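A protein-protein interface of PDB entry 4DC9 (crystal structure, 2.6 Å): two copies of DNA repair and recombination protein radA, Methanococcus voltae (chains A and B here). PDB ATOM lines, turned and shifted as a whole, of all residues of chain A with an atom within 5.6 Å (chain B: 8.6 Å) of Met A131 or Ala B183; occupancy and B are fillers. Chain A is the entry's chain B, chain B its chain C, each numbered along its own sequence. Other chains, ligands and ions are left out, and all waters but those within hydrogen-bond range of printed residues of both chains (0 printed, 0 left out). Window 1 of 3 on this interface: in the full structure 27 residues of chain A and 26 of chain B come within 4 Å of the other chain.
Arg A125 touches none of the printed residues of chain B.
Printed residues of chain B within 4 Å of Met A131: Ala B183.
Of the printed residues of chain A, Gly B7 touches Phe A135 (3.8 Å).
Of chain A, only Tyr A127 (3.7 Å) and Met A131 (3.6 Å) come within 4 Å of Ala B183.
Printed residues of chain A within 4 Å of Asn B186: Tyr A127.
Printed residues of chain A within 4 Å of Ile B221: Tyr A127.
The nearest residue of chain B that does not touch Met A131 is Gly B179 (5.8 Å).
2 positions are printed for both chains.
OD1 of Asn A128 is in hydrogen-bond range of N of Arg B180 (3.4 Å).
The side-chain carboxylate (OD2) of Asp A130 lies within salt-bridge range of the guanidinium group (NH2) of Arg B180.
Of the 26 printed residues of chain B, 9 touch a printed residue of chain A.
Hydrophobic or aromatic side chains of chain B that line the printed part of chain A: Phe B8, Ala B183, Ile B221 and Ala B225.
Hydrophobic or aromatic side chains of chain A within 4 Å of the printed part of chain B: Tyr A127, Met A131 and Phe A135.
Ala B183 touches Tyr A127.
CB of Asn B186 touches OH of Tyr A127 (3.2 Å).
Tyr A127 touches Ile B221 (O to CD1, 3.3 Å).
Tyr A127 touches Ala B225.
OD1 of Asn A128 touches O of Gln B176 (3.9 Å).
Asn A128 touches Gly B179 (OD1 to C, 3.6 Å).
OG of Ser A129 touches OE1 of Gln B176, at 3.9 Å.
SD of Met A131 touches CB of Ala B183 (3.6 Å).
Phe A135 touches Gly B7 (CE2 to CA, 3.8 Å).
Phe A135 touches Phe B8.
ND2 of Asn A128 lies close to N of Met A131, at 3.0 Å.
The backbone carbonyl oxygen of Met B182 is in hydrogen-bond range of the side-chain amide nitrogen of Asn B186 (2.8 Å).
The side-chain amide nitrogen of Asn B186 sits at hydrogen-bond distance from the backbone carbonyl oxygen of Ala B225, at 3.2 Å.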
ATOM      1  N   ARG A 125      -4.471  13.884  -8.041  1.00  0.00           N
ATOM      2  CA  ARG A 125      -3.746  14.959  -8.662  1.00  0.00           C
ATOM      3  C   ARG A 125      -3.587  14.585 -10.127  1.00  0.00           C
ATOM      4  O   ARG A 125      -3.159  13.476 -10.459  1.00  0.00           O
ATOM      5  CB  ARG A 125      -2.422  15.202  -7.919  1.00  0.00           C
ATOM      6  CG  ARG A 125      -1.531  16.348  -8.412  1.00  0.00           C
ATOM      7  CD  ARG A 125      -2.043  17.780  -8.240  1.00  0.00           C
ATOM      8  NE  ARG A 125      -2.030  18.384  -9.576  1.00  0.00           N
ATOM      9  CZ  ARG A 125      -1.230  19.367  -9.976  1.00  0.00           C
ATOM     10  NH1 ARG A 125      -0.383  19.943  -9.131  1.00  0.00           N
ATOM     11  NH2 ARG A 125      -1.292  19.796 -11.226  1.00  0.00           N
ATOM     12  N   ALA A 126      -3.998  15.491 -11.008  1.00  0.00           N
ATOM     13  CA  ALA A 126      -4.010  15.235 -12.463  1.00  0.00           C
ATOM     14  C   ALA A 126      -3.174  16.319 -13.103  1.00  0.00           C
ATOM     15  O   ALA A 126      -3.120  17.447 -12.605  1.00  0.00           O
ATOM     16  CB  ALA A 126      -5.429  15.245 -13.007  1.00  0.00           C
ATOM     17  N   TYR A 127      -2.482  15.975 -14.175  1.00  0.00           N
ATOM     18  CA  TYR A 127      -1.534  16.915 -14.772  1.00  0.00           C
ATOM     19  C   TYR A 127      -1.886  17.123 -16.223  1.00  0.00           C
ATOM     20  O   TYR A 127      -1.170  17.825 -16.963  1.00  0.00           O
ATOM     21  CB  TYR A 127      -0.088  16.410 -14.656  1.00  0.00           C
ATOM     22  CG  TYR A 127       0.335  16.104 -13.256  1.00  0.00           C
ATOM     23  CD1 TYR A 127       0.844  17.109 -12.431  1.00  0.00           C
ATOM     24  CD2 TYR A 127       0.237  14.815 -12.737  1.00  0.00           C
ATOM     25  CE1 TYR A 127       1.250  16.846 -11.124  1.00  0.00           C
ATOM     26  CE2 TYR A 127       0.630  14.544 -11.417  1.00  0.00           C
ATOM     27  CZ  TYR A 127       1.134  15.566 -10.618  1.00  0.00           C
ATOM     28  OH  TYR A 127       1.522  15.327  -9.316  1.00  0.00           O
ATOM     29  N   ASN A 128      -2.981  16.486 -16.623  1.00  0.00           N
ATOM     30  CA  ASN A 128      -3.453  16.571 -17.979  1.00  0.00           C
ATOM     31  C   ASN A 128      -4.767  15.903 -18.135  1.00  0.00           C
ATOM     32  O   ASN A 128      -5.154  15.081 -17.291  1.00  0.00           O
ATOM     33  CB  ASN A 128      -2.452  15.957 -18.950  1.00  0.00           C
ATOM     34  CG  ASN A 128      -2.271  14.450 -18.771  1.00  0.00           C
ATOM     35  OD1 ASN A 128      -1.359  13.898 -19.375  1.00  0.00           O
ATOM     36  ND2 ASN A 128      -3.124  13.779 -17.979  1.00  0.00           N
ATOM     37  N   SER A 129      -5.417  16.240 -19.253  1.00  0.00           N
ATOM     38  CA  SER A 129      -6.767  15.794 -19.600  1.00  0.00           C
ATOM     39  C   SER A 129      -6.943  14.330 -19.380  1.00  0.00           C
ATOM     40  O   SER A 129      -7.881  13.939 -18.703  1.00  0.00           O
ATOM     41  CB  SER A 129      -7.135  16.152 -21.049  1.00  0.00           C
ATOM     42  OG  SER A 129      -6.005  16.086 -21.899  1.00  0.00           O
ATOM     43  N   ASP A 130      -6.036  13.520 -19.930  1.00  0.00           N
ATOM     44  CA  ASP A 130      -6.202  12.061 -19.842  1.00  0.00           C
ATOM     45  C   ASP A 130      -6.392  11.635 -18.383  1.00  0.00           C
ATOM     46  O   ASP A 130      -7.467  11.135 -18.014  1.00  0.00           O
ATOM     47  CB  ASP A 130      -5.061  11.299 -20.526  1.00  0.00           C
ATOM     48  CG  ASP A 130      -5.034  11.487 -22.047  1.00  0.00           C
ATOM     49  OD1 ASP A 130      -6.103  11.458 -22.715  1.00  0.00           O
ATOM     50  OD2 ASP A 130      -3.914  11.642 -22.587  1.00  0.00           O
ATOM     51  N   MET A 131      -5.373  11.871 -17.550  1.00  0.00           N
ATOM     52  CA  MET A 131      -5.476  11.606 -16.099  1.00  0.00           C
ATOM     53  C   MET A 131      -6.744  12.182 -15.484  1.00  0.00           C
ATOM     54  O   MET A 131      -7.451  11.488 -14.743  1.00  0.00           O
ATOM     55  CB  MET A 131      -4.281  12.176 -15.356  1.00  0.00           C
ATOM     56  CG  MET A 131      -3.034  11.337 -15.438  1.00  0.00           C
ATOM     57  SD  MET A 131      -1.791  12.203 -14.503  1.00  0.00           S
ATOM     58  CE  MET A 131      -2.109  11.675 -12.808  1.00  0.00           C
ATOM     59  N   GLN A 132      -7.040  13.441 -15.805  1.00  0.00           N
ATOM     60  CA  GLN A 132      -8.302  14.063 -15.337  1.00  0.00           C
ATOM     61  C   GLN A 132      -9.556  13.204 -15.636  1.00  0.00           C
ATOM     62  O   GLN A 132     -10.378  12.941 -14.760  1.00  0.00           O
ATOM     63  CB  GLN A 132      -8.485  15.501 -15.899  1.00  0.00           C
ATOM     64  CG  GLN A 132      -9.713  16.188 -15.322  1.00  0.00           C
ATOM     65  CD  GLN A 132      -9.937  17.561 -15.865  1.00  0.00           C
ATOM     66  OE1 GLN A 132      -8.990  18.290 -16.149  1.00  0.00           O
ATOM     67  NE2 GLN A 132     -11.206  17.938 -16.018  1.00  0.00           N
ATOM     68  N   MET A 133      -9.663  12.768 -16.883  1.00  0.00           N
ATOM     69  CA  MET A 133     -10.802  12.020 -17.363  1.00  0.00           C
ATOM     70  C   MET A 133     -10.853  10.669 -16.723  1.00  0.00           C
ATOM     71  O   MET A 133     -11.929  10.205 -16.276  1.00  0.00           O
ATOM     72  CB  MET A 133     -10.684  11.878 -18.874  1.00  0.00           C
ATOM     73  CG  MET A 133     -10.721  13.235 -19.539  1.00  0.00           C
ATOM     74  SD  MET A 133     -11.153  13.243 -21.269  1.00  0.00           S
ATOM     75  CE  MET A 133     -12.667  12.273 -21.272  1.00  0.00           C
ATOM     76  N   LEU A 134      -9.672  10.057 -16.652  1.00  0.00           N
ATOM     77  CA  LEU A 134      -9.538   8.710 -16.133  1.00  0.00           C
ATOM     78  C   LEU A 134      -9.930   8.679 -14.694  1.00  0.00           C
ATOM     79  O   LEU A 134     -10.700   7.816 -14.301  1.00  0.00           O
ATOM     80  CB  LEU A 134      -8.112   8.217 -16.291  1.00  0.00           C
ATOM     81  CG  LEU A 134      -7.831   6.731 -16.031  1.00  0.00           C
ATOM     82  CD1 LEU A 134      -8.914   5.778 -16.558  1.00  0.00           C
ATOM     83  CD2 LEU A 134      -6.467   6.405 -16.616  1.00  0.00           C
ATOM     84  N   PHE A 135      -9.457   9.643 -13.901  1.00  0.00           N
ATOM     85  CA  PHE A 135      -9.810   9.604 -12.474  1.00  0.00           C
ATOM     86  C   PHE A 135     -11.305   9.632 -12.312  1.00  0.00           C
ATOM     87  O   PHE A 135     -11.866   8.942 -11.478  1.00  0.00           O
ATOM     88  CB  PHE A 135      -9.193  10.740 -11.690  1.00  0.00           C
ATOM     89  CG  PHE A 135      -7.747  10.560 -11.420  1.00  0.00           C
ATOM     90  CD1 PHE A 135      -6.842  11.545 -11.763  1.00  0.00           C
ATOM     91  CD2 PHE A 135      -7.280   9.401 -10.814  1.00  0.00           C
ATOM     92  CE1 PHE A 135      -5.485  11.383 -11.510  1.00  0.00           C
ATOM     93  CE2 PHE A 135      -5.927   9.224 -10.558  1.00  0.00           C
ATOM     94  CZ  PHE A 135      -5.027  10.219 -10.903  1.00  0.00           C
ATOM     95  N   ALA A 136     -11.952  10.435 -13.145  1.00  0.00           N
ATOM     96  CA  ALA A 136     -13.391  10.597 -13.052  1.00  0.00           C
ATOM     97  C   ALA A 136     -14.076   9.310 -13.493  1.00  0.00           C
ATOM     98  O   ALA A 136     -15.090   8.922 -12.894  1.00  0.00           O
ATOM     99  CB  ALA A 136     -13.851  11.797 -13.861  1.00  0.00           C
ATOM    100  N   LEU B   6      -5.421   2.630  -7.288  1.00  0.00           N
ATOM    101  CA  LEU B   6      -5.973   3.403  -8.432  1.00  0.00           C
ATOM    102  C   LEU B   6      -5.200   4.728  -8.763  1.00  0.00           C
ATOM    103  O   LEU B   6      -4.635   4.884  -9.862  1.00  0.00           O
ATOM    104  CB  LEU B   6      -7.496   3.639  -8.225  1.00  0.00           C
ATOM    105  CG  LEU B   6      -8.471   2.437  -8.152  1.00  0.00           C
ATOM    106  CD1 LEU B   6      -9.348   2.496  -6.910  1.00  0.00           C
ATOM    107  CD2 LEU B   6      -9.333   2.289  -9.407  1.00  0.00           C
ATOM    108  N   GLY B   7      -5.177   5.665  -7.816  1.00  0.00           N
ATOM    109  CA  GLY B   7      -4.377   6.888  -7.932  1.00  0.00           C
ATOM    110  C   GLY B   7      -4.848   7.939  -6.945  1.00  0.00           C
ATOM    111  O   GLY B   7      -4.358   9.063  -6.932  1.00  0.00           O
ATOM    112  N   PHE B   8      -5.815   7.567  -6.114  1.00  0.00           N
ATOM    113  CA  PHE B   8      -6.418   8.490  -5.164  1.00  0.00           C
ATOM    114  C   PHE B   8      -5.680   8.351  -3.846  1.00  0.00           C
ATOM    115  O   PHE B   8      -5.701   7.274  -3.239  1.00  0.00           O
ATOM    116  CB  PHE B   8      -7.904   8.147  -4.927  1.00  0.00           C
ATOM    117  CG  PHE B   8      -8.754   8.131  -6.174  1.00  0.00           C
ATOM    118  CD1 PHE B   8      -9.676   9.139  -6.407  1.00  0.00           C
ATOM    119  CD2 PHE B   8      -8.652   7.089  -7.097  1.00  0.00           C
ATOM    120  CE1 PHE B   8     -10.460   9.131  -7.552  1.00  0.00           C
ATOM    121  CE2 PHE B   8      -9.434   7.072  -8.240  1.00  0.00           C
ATOM    122  CZ  PHE B   8     -10.341   8.095  -8.468  1.00  0.00           C
ATOM    123  N   VAL B  44       9.053  17.958  -7.504  1.00  0.00           N
ATOM    124  CA  VAL B  44       9.848  18.227  -8.719  1.00  0.00           C
ATOM    125  C   VAL B  44      10.406  19.637  -8.636  1.00  0.00           C
ATOM    126  O   VAL B  44       9.744  20.573  -8.255  1.00  0.00           O
ATOM    127  CB  VAL B  44       9.021  18.056 -10.027  1.00  0.00           C
ATOM    128  CG1 VAL B  44       9.881  18.308 -11.258  1.00  0.00           C
ATOM    129  CG2 VAL B  44       8.433  16.659 -10.114  1.00  0.00           C
ATOM    130  N   MET B 133      10.980   9.871 -22.262  1.00  0.00           N
ATOM    131  CA  MET B 133       9.827   9.474 -21.450  1.00  0.00           C
ATOM    132  C   MET B 133       9.923   8.048 -20.991  1.00  0.00           C
ATOM    133  O   MET B 133       9.463   7.702 -19.911  1.00  0.00           O
ATOM    134  CB  MET B 133       8.543   9.665 -22.218  1.00  0.00           C
ATOM    135  CG  MET B 133       8.205  11.137 -22.382  1.00  0.00           C
ATOM    136  SD  MET B 133       6.815  11.388 -23.488  1.00  0.00           S
ATOM    137  CE  MET B 133       5.540  10.325 -22.765  1.00  0.00           C
ATOM    138  N   ALA B 136      12.281   7.343 -18.276  1.00  0.00           N
ATOM    139  CA  ALA B 136      11.699   7.792 -17.036  1.00  0.00           C
ATOM    140  C   ALA B 136      10.805   6.699 -16.437  1.00  0.00           C
ATOM    141  O   ALA B 136      10.837   6.439 -15.219  1.00  0.00           O
ATOM    142  CB  ALA B 136      10.925   9.069 -17.287  1.00  0.00           C
ATOM    143  N   GLU B 137      10.041   6.041 -17.306  1.00  0.00           N
ATOM    144  CA  GLU B 137       9.151   4.940 -16.912  1.00  0.00           C
ATOM    145  C   GLU B 137       9.953   3.730 -16.448  1.00  0.00           C
ATOM    146  O   GLU B 137       9.581   3.036 -15.509  1.00  0.00           O
ATOM    147  CB  GLU B 137       8.212   4.547 -18.067  1.00  0.00           C
ATOM    148  CG  GLU B 137       7.074   5.527 -18.294  1.00  0.00           C
ATOM    149  CD  GLU B 137       6.410   5.366 -19.643  1.00  0.00           C
ATOM    150  OE1 GLU B 137       5.814   6.346 -20.154  1.00  0.00           O
ATOM    151  OE2 GLU B 137       6.467   4.256 -20.205  1.00  0.00           O
ATOM    152  N   GLN B 176       0.400  17.411 -24.631  1.00  0.00           N
ATOM    153  CA  GLN B 176      -0.164  16.237 -23.962  1.00  0.00           C
ATOM    154  C   GLN B 176       0.966  15.279 -23.544  1.00  0.00           C
ATOM    155  O   GLN B 176       0.944  14.694 -22.430  1.00  0.00           O
ATOM    156  CB  GLN B 176      -1.190  15.514 -24.864  1.00  0.00           C
ATOM    157  CG  GLN B 176      -2.273  16.382 -25.534  1.00  0.00           C
ATOM    158  CD  GLN B 176      -3.454  15.562 -26.093  1.00  0.00           C
ATOM    159  OE1 GLN B 176      -4.417  15.301 -25.379  1.00  0.00           O
ATOM    160  NE2 GLN B 176      -3.382  15.163 -27.362  1.00  0.00           N
ATOM    161  N   LYS B 177       1.950  15.144 -24.441  1.00  0.00           N
ATOM    162  CA  LYS B 177       3.096  14.248 -24.234  1.00  0.00           C
ATOM    163  C   LYS B 177       3.918  14.715 -23.022  1.00  0.00           C
ATOM    164  O   LYS B 177       4.299  13.912 -22.164  1.00  0.00           O
ATOM    165  CB  LYS B 177       3.969  14.194 -25.489  1.00  0.00           C
ATOM    166  CG  LYS B 177       4.482  12.803 -25.856  1.00  0.00           C
ATOM    167  CD  LYS B 177       5.282  12.838 -27.162  1.00  0.00           C
ATOM    168  CE  LYS B 177       6.104  11.565 -27.319  1.00  0.00           C
ATOM    169  NZ  LYS B 177       6.924  11.514 -28.558  1.00  0.00           N
ATOM    170  N   LEU B 178       4.152  16.022 -22.989  1.00  0.00           N
ATOM    171  CA  LEU B 178       4.771  16.715 -21.891  1.00  0.00           C
ATOM    172  C   LEU B 178       4.049  16.443 -20.618  1.00  0.00           C
ATOM    173  O   LEU B 178       4.653  16.049 -19.622  1.00  0.00           O
ATOM    174  CB  LEU B 178       4.685  18.189 -22.157  1.00  0.00           C
ATOM    175  CG  LEU B 178       5.912  18.989 -21.801  1.00  0.00           C
ATOM    176  CD1 LEU B 178       7.129  18.092 -21.758  1.00  0.00           C
ATOM    177  CD2 LEU B 178       6.043  19.983 -22.932  1.00  0.00           C
ATOM    178  N   GLY B 179       2.740  16.648 -20.665  1.00  0.00           N
ATOM    179  CA  GLY B 179       1.865  16.389 -19.538  1.00  0.00           C
ATOM    180  C   GLY B 179       2.036  14.984 -19.071  1.00  0.00           C
ATOM    181  O   GLY B 179       2.198  14.731 -17.862  1.00  0.00           O
ATOM    182  N   ARG B 180       2.025  14.049 -20.021  1.00  0.00           N
ATOM    183  CA  ARG B 180       2.116  12.629 -19.638  1.00  0.00           C
ATOM    184  C   ARG B 180       3.427  12.296 -18.947  1.00  0.00           C
ATOM    185  O   ARG B 180       3.425  11.554 -17.981  1.00  0.00           O
ATOM    186  CB  ARG B 180       1.879  11.687 -20.812  1.00  0.00           C
ATOM    187  CG  ARG B 180       1.802  10.231 -20.375  1.00  0.00           C
ATOM    188  CD  ARG B 180       0.932   9.405 -21.293  1.00  0.00           C
ATOM    189  NE  ARG B 180       1.080   9.832 -22.680  1.00  0.00           N
ATOM    190  CZ  ARG B 180       0.159  10.507 -23.374  1.00  0.00           C
ATOM    191  NH1 ARG B 180       0.405  10.856 -24.637  1.00  0.00           N
ATOM    192  NH2 ARG B 180      -1.004  10.836 -22.812  1.00  0.00           N
ATOM    193  N   HIS B 181       4.526  12.842 -19.466  1.00  0.00           N
ATOM    194  CA  HIS B 181       5.864  12.742 -18.871  1.00  0.00           C
ATOM    195  C   HIS B 181       5.842  13.366 -17.506  1.00  0.00           C
ATOM    196  O   HIS B 181       6.190  12.752 -16.519  1.00  0.00           O
ATOM    197  CB  HIS B 181       6.848  13.473 -19.777  1.00  0.00           C
ATOM    198  CG  HIS B 181       8.299  13.251 -19.445  1.00  0.00           C
ATOM    199  ND1 HIS B 181       9.226  14.257 -19.507  1.00  0.00           N
ATOM    200  CD2 HIS B 181       8.993  12.094 -19.072  1.00  0.00           C
ATOM    201  CE1 HIS B 181      10.440  13.762 -19.191  1.00  0.00           C
ATOM    202  NE2 HIS B 181      10.293  12.435 -18.914  1.00  0.00           N
ATOM    203  N   MET B 182       5.376  14.590 -17.437  1.00  0.00           N
ATOM    204  CA  MET B 182       5.278  15.281 -16.184  1.00  0.00           C
ATOM    205  C   MET B 182       4.562  14.489 -15.101  1.00  0.00           C
ATOM    206  O   MET B 182       4.940  14.570 -13.928  1.00  0.00           O
ATOM    207  CB  MET B 182       4.575  16.609 -16.408  1.00  0.00           C
ATOM    208  CG  MET B 182       5.441  17.575 -17.218  1.00  0.00           C
ATOM    209  SD  MET B 182       6.904  18.169 -16.316  1.00  0.00           S
ATOM    210  CE  MET B 182       6.054  18.850 -14.894  1.00  0.00           C
ATOM    211  N   ALA B 183       3.522  13.743 -15.481  1.00  0.00           N
ATOM    212  CA  ALA B 183       2.845  12.869 -14.516  1.00  0.00           C
ATOM    213  C   ALA B 183       3.871  11.913 -13.955  1.00  0.00           C
ATOM    214  O   ALA B 183       4.085  11.850 -12.742  1.00  0.00           O
ATOM    215  CB  ALA B 183       1.729  12.075 -15.168  1.00  0.00           C
ATOM    216  N   THR B 184       4.522  11.185 -14.857  1.00  0.00           N
ATOM    217  CA  THR B 184       5.470  10.150 -14.482  1.00  0.00           C
ATOM    218  C   THR B 184       6.453  10.694 -13.447  1.00  0.00           C
ATOM    219  O   THR B 184       6.668  10.094 -12.398  1.00  0.00           O
ATOM    220  CB  THR B 184       6.226   9.622 -15.707  1.00  0.00           C
ATOM    221  OG1 THR B 184       5.324   8.845 -16.503  1.00  0.00           O
ATOM    222  CG2 THR B 184       7.384   8.744 -15.269  1.00  0.00           C
ATOM    223  N   LEU B 185       7.007  11.858 -13.753  1.00  0.00           N
ATOM    224  CA  LEU B 185       8.008  12.439 -12.932  1.00  0.00           C
ATOM    225  C   LEU B 185       7.476  12.672 -11.501  1.00  0.00           C
ATOM    226  O   LEU B 185       8.119  12.326 -10.519  1.00  0.00           O
ATOM    227  CB  LEU B 185       8.480  13.721 -13.599  1.00  0.00           C
ATOM    228  CG  LEU B 185       9.337  13.573 -14.856  1.00  0.00           C
ATOM    229  CD1 LEU B 185       9.886  14.957 -15.169  1.00  0.00           C
ATOM    230  CD2 LEU B 185      10.496  12.578 -14.704  1.00  0.00           C
ATOM    231  N   ASN B 186       6.296  13.250 -11.395  1.00  0.00           N
ATOM    232  CA  ASN B 186       5.629  13.388 -10.129  1.00  0.00           C
ATOM    233  C   ASN B 186       5.273  12.051  -9.464  1.00  0.00           C
ATOM    234  O   ASN B 186       5.558  11.845  -8.286  1.00  0.00           O
ATOM    235  CB  ASN B 186       4.363  14.210 -10.336  1.00  0.00           C
ATOM    236  CG  ASN B 186       4.656  15.673 -10.558  1.00  0.00           C
ATOM    237  OD1 ASN B 186       5.159  16.325  -9.671  1.00  0.00           O
ATOM    238  ND2 ASN B 186       4.344  16.193 -11.750  1.00  0.00           N
ATOM    239  N   LYS B 187       4.642  11.148 -10.214  1.00  0.00           N
ATOM    240  CA  LYS B 187       4.263   9.834  -9.670  1.00  0.00           C
ATOM    241  C   LYS B 187       5.470   9.173  -9.003  1.00  0.00           C
ATOM    242  O   LYS B 187       5.384   8.691  -7.876  1.00  0.00           O
ATOM    243  CB  LYS B 187       3.637   8.945 -10.759  1.00  0.00           C
ATOM    244  CG  LYS B 187       3.865   7.445 -10.611  1.00  0.00           C
ATOM    245  CD  LYS B 187       3.844   6.753 -11.973  1.00  0.00           C
ATOM    246  CE  LYS B 187       4.493   5.370 -11.939  1.00  0.00           C
ATOM    247  NZ  LYS B 187       3.724   4.389 -12.767  1.00  0.00           N
ATOM    248  N   LEU B 188       6.606   9.201  -9.676  1.00  0.00           N
ATOM    249  CA  LEU B 188       7.734   8.473  -9.184  1.00  0.00           C
ATOM    250  C   LEU B 188       8.535   9.228  -8.107  1.00  0.00           C
ATOM    251  O   LEU B 188       9.324   8.627  -7.389  1.00  0.00           O
ATOM    252  CB  LEU B 188       8.586   7.919 -10.346  1.00  0.00           C
ATOM    253  CG  LEU B 188       9.646   8.744 -11.028  1.00  0.00           C
ATOM    254  CD1 LEU B 188      10.897   8.684 -10.187  1.00  0.00           C
ATOM    255  CD2 LEU B 188       9.932   8.204 -12.414  1.00  0.00           C
ATOM    256  N   ALA B 189       8.321  10.530  -7.976  1.00  0.00           N
ATOM    257  CA  ALA B 189       8.858  11.256  -6.830  1.00  0.00           C
ATOM    258  C   ALA B 189       8.039  10.858  -5.621  1.00  0.00           C
ATOM    259  O   ALA B 189       8.567  10.712  -4.512  1.00  0.00           O
ATOM    260  CB  ALA B 189       8.735  12.749  -7.038  1.00  0.00           C
ATOM    261  N   ASP B 190       6.742  10.681  -5.852  1.00  0.00           N
ATOM    262  CA  ASP B 190       5.768  10.646  -4.780  1.00  0.00           C
ATOM    263  C   ASP B 190       5.585   9.221  -4.291  1.00  0.00           C
ATOM    264  O   ASP B 190       5.241   9.007  -3.130  1.00  0.00           O
ATOM    265  CB  ASP B 190       4.418  11.269  -5.218  1.00  0.00           C
ATOM    266  CG  ASP B 190       4.385  12.813  -5.078  1.00  0.00           C
ATOM    267  OD1 ASP B 190       5.373  13.490  -5.430  1.00  0.00           O
ATOM    268  OD2 ASP B 190       3.357  13.368  -4.634  1.00  0.00           O
ATOM    269  N   LEU B 191       5.805   8.254  -5.172  1.00  0.00           N
ATOM    270  CA  LEU B 191       5.554   6.857  -4.834  1.00  0.00           C
ATOM    271  C   LEU B 191       6.844   6.131  -4.488  1.00  0.00           C
ATOM    272  O   LEU B 191       6.821   5.020  -3.973  1.00  0.00           O
ATOM    273  CB  LEU B 191       4.756   6.136  -5.946  1.00  0.00           C
ATOM    274  CG  LEU B 191       3.281   6.615  -6.055  1.00  0.00           C
ATOM    275  CD1 LEU B 191       2.539   6.179  -7.331  1.00  0.00           C
ATOM    276  CD2 LEU B 191       2.487   6.266  -4.793  1.00  0.00           C
ATOM    277  N   VAL B 196      13.219  14.690  -7.726  1.00  0.00           N
ATOM    278  CA  VAL B 196      13.314  14.823  -9.152  1.00  0.00           C
ATOM    279  C   VAL B 196      13.628  16.246  -9.520  1.00  0.00           C
ATOM    280  O   VAL B 196      12.854  17.157  -9.169  1.00  0.00           O
ATOM    281  CB  VAL B 196      11.991  14.510  -9.811  1.00  0.00           C
ATOM    282  CG1 VAL B 196      12.148  14.631 -11.337  1.00  0.00           C
ATOM    283  CG2 VAL B 196      11.493  13.140  -9.351  1.00  0.00           C
ATOM    284  N   ILE B 221       1.479  23.616 -18.679  1.00  0.00           N
ATOM    285  CA  ILE B 221       1.346  22.174 -18.461  1.00  0.00           C
ATOM    286  C   ILE B 221       2.514  21.695 -17.561  1.00  0.00           C
ATOM    287  O   ILE B 221       2.369  20.787 -16.706  1.00  0.00           O
ATOM    288  CB  ILE B 221       1.238  21.427 -19.829  1.00  0.00           C
ATOM    289  CG1 ILE B 221      -0.218  20.966 -20.130  1.00  0.00           C
ATOM    290  CG2 ILE B 221       2.227  20.277 -19.957  1.00  0.00           C
ATOM    291  CD1 ILE B 221      -1.059  20.374 -19.001  1.00  0.00           C
ATOM    292  N   ALA B 225       2.565  21.320 -12.974  1.00  0.00           N
ATOM    293  CA  ALA B 225       3.141  20.058 -12.474  1.00  0.00           C
ATOM    294  C   ALA B 225       4.533  20.207 -11.824  1.00  0.00           C
ATOM    295  O   ALA B 225       5.106  19.233 -11.365  1.00  0.00           O
ATOM    296  CB  ALA B 225       3.203  19.018 -13.577  1.00  0.00           C
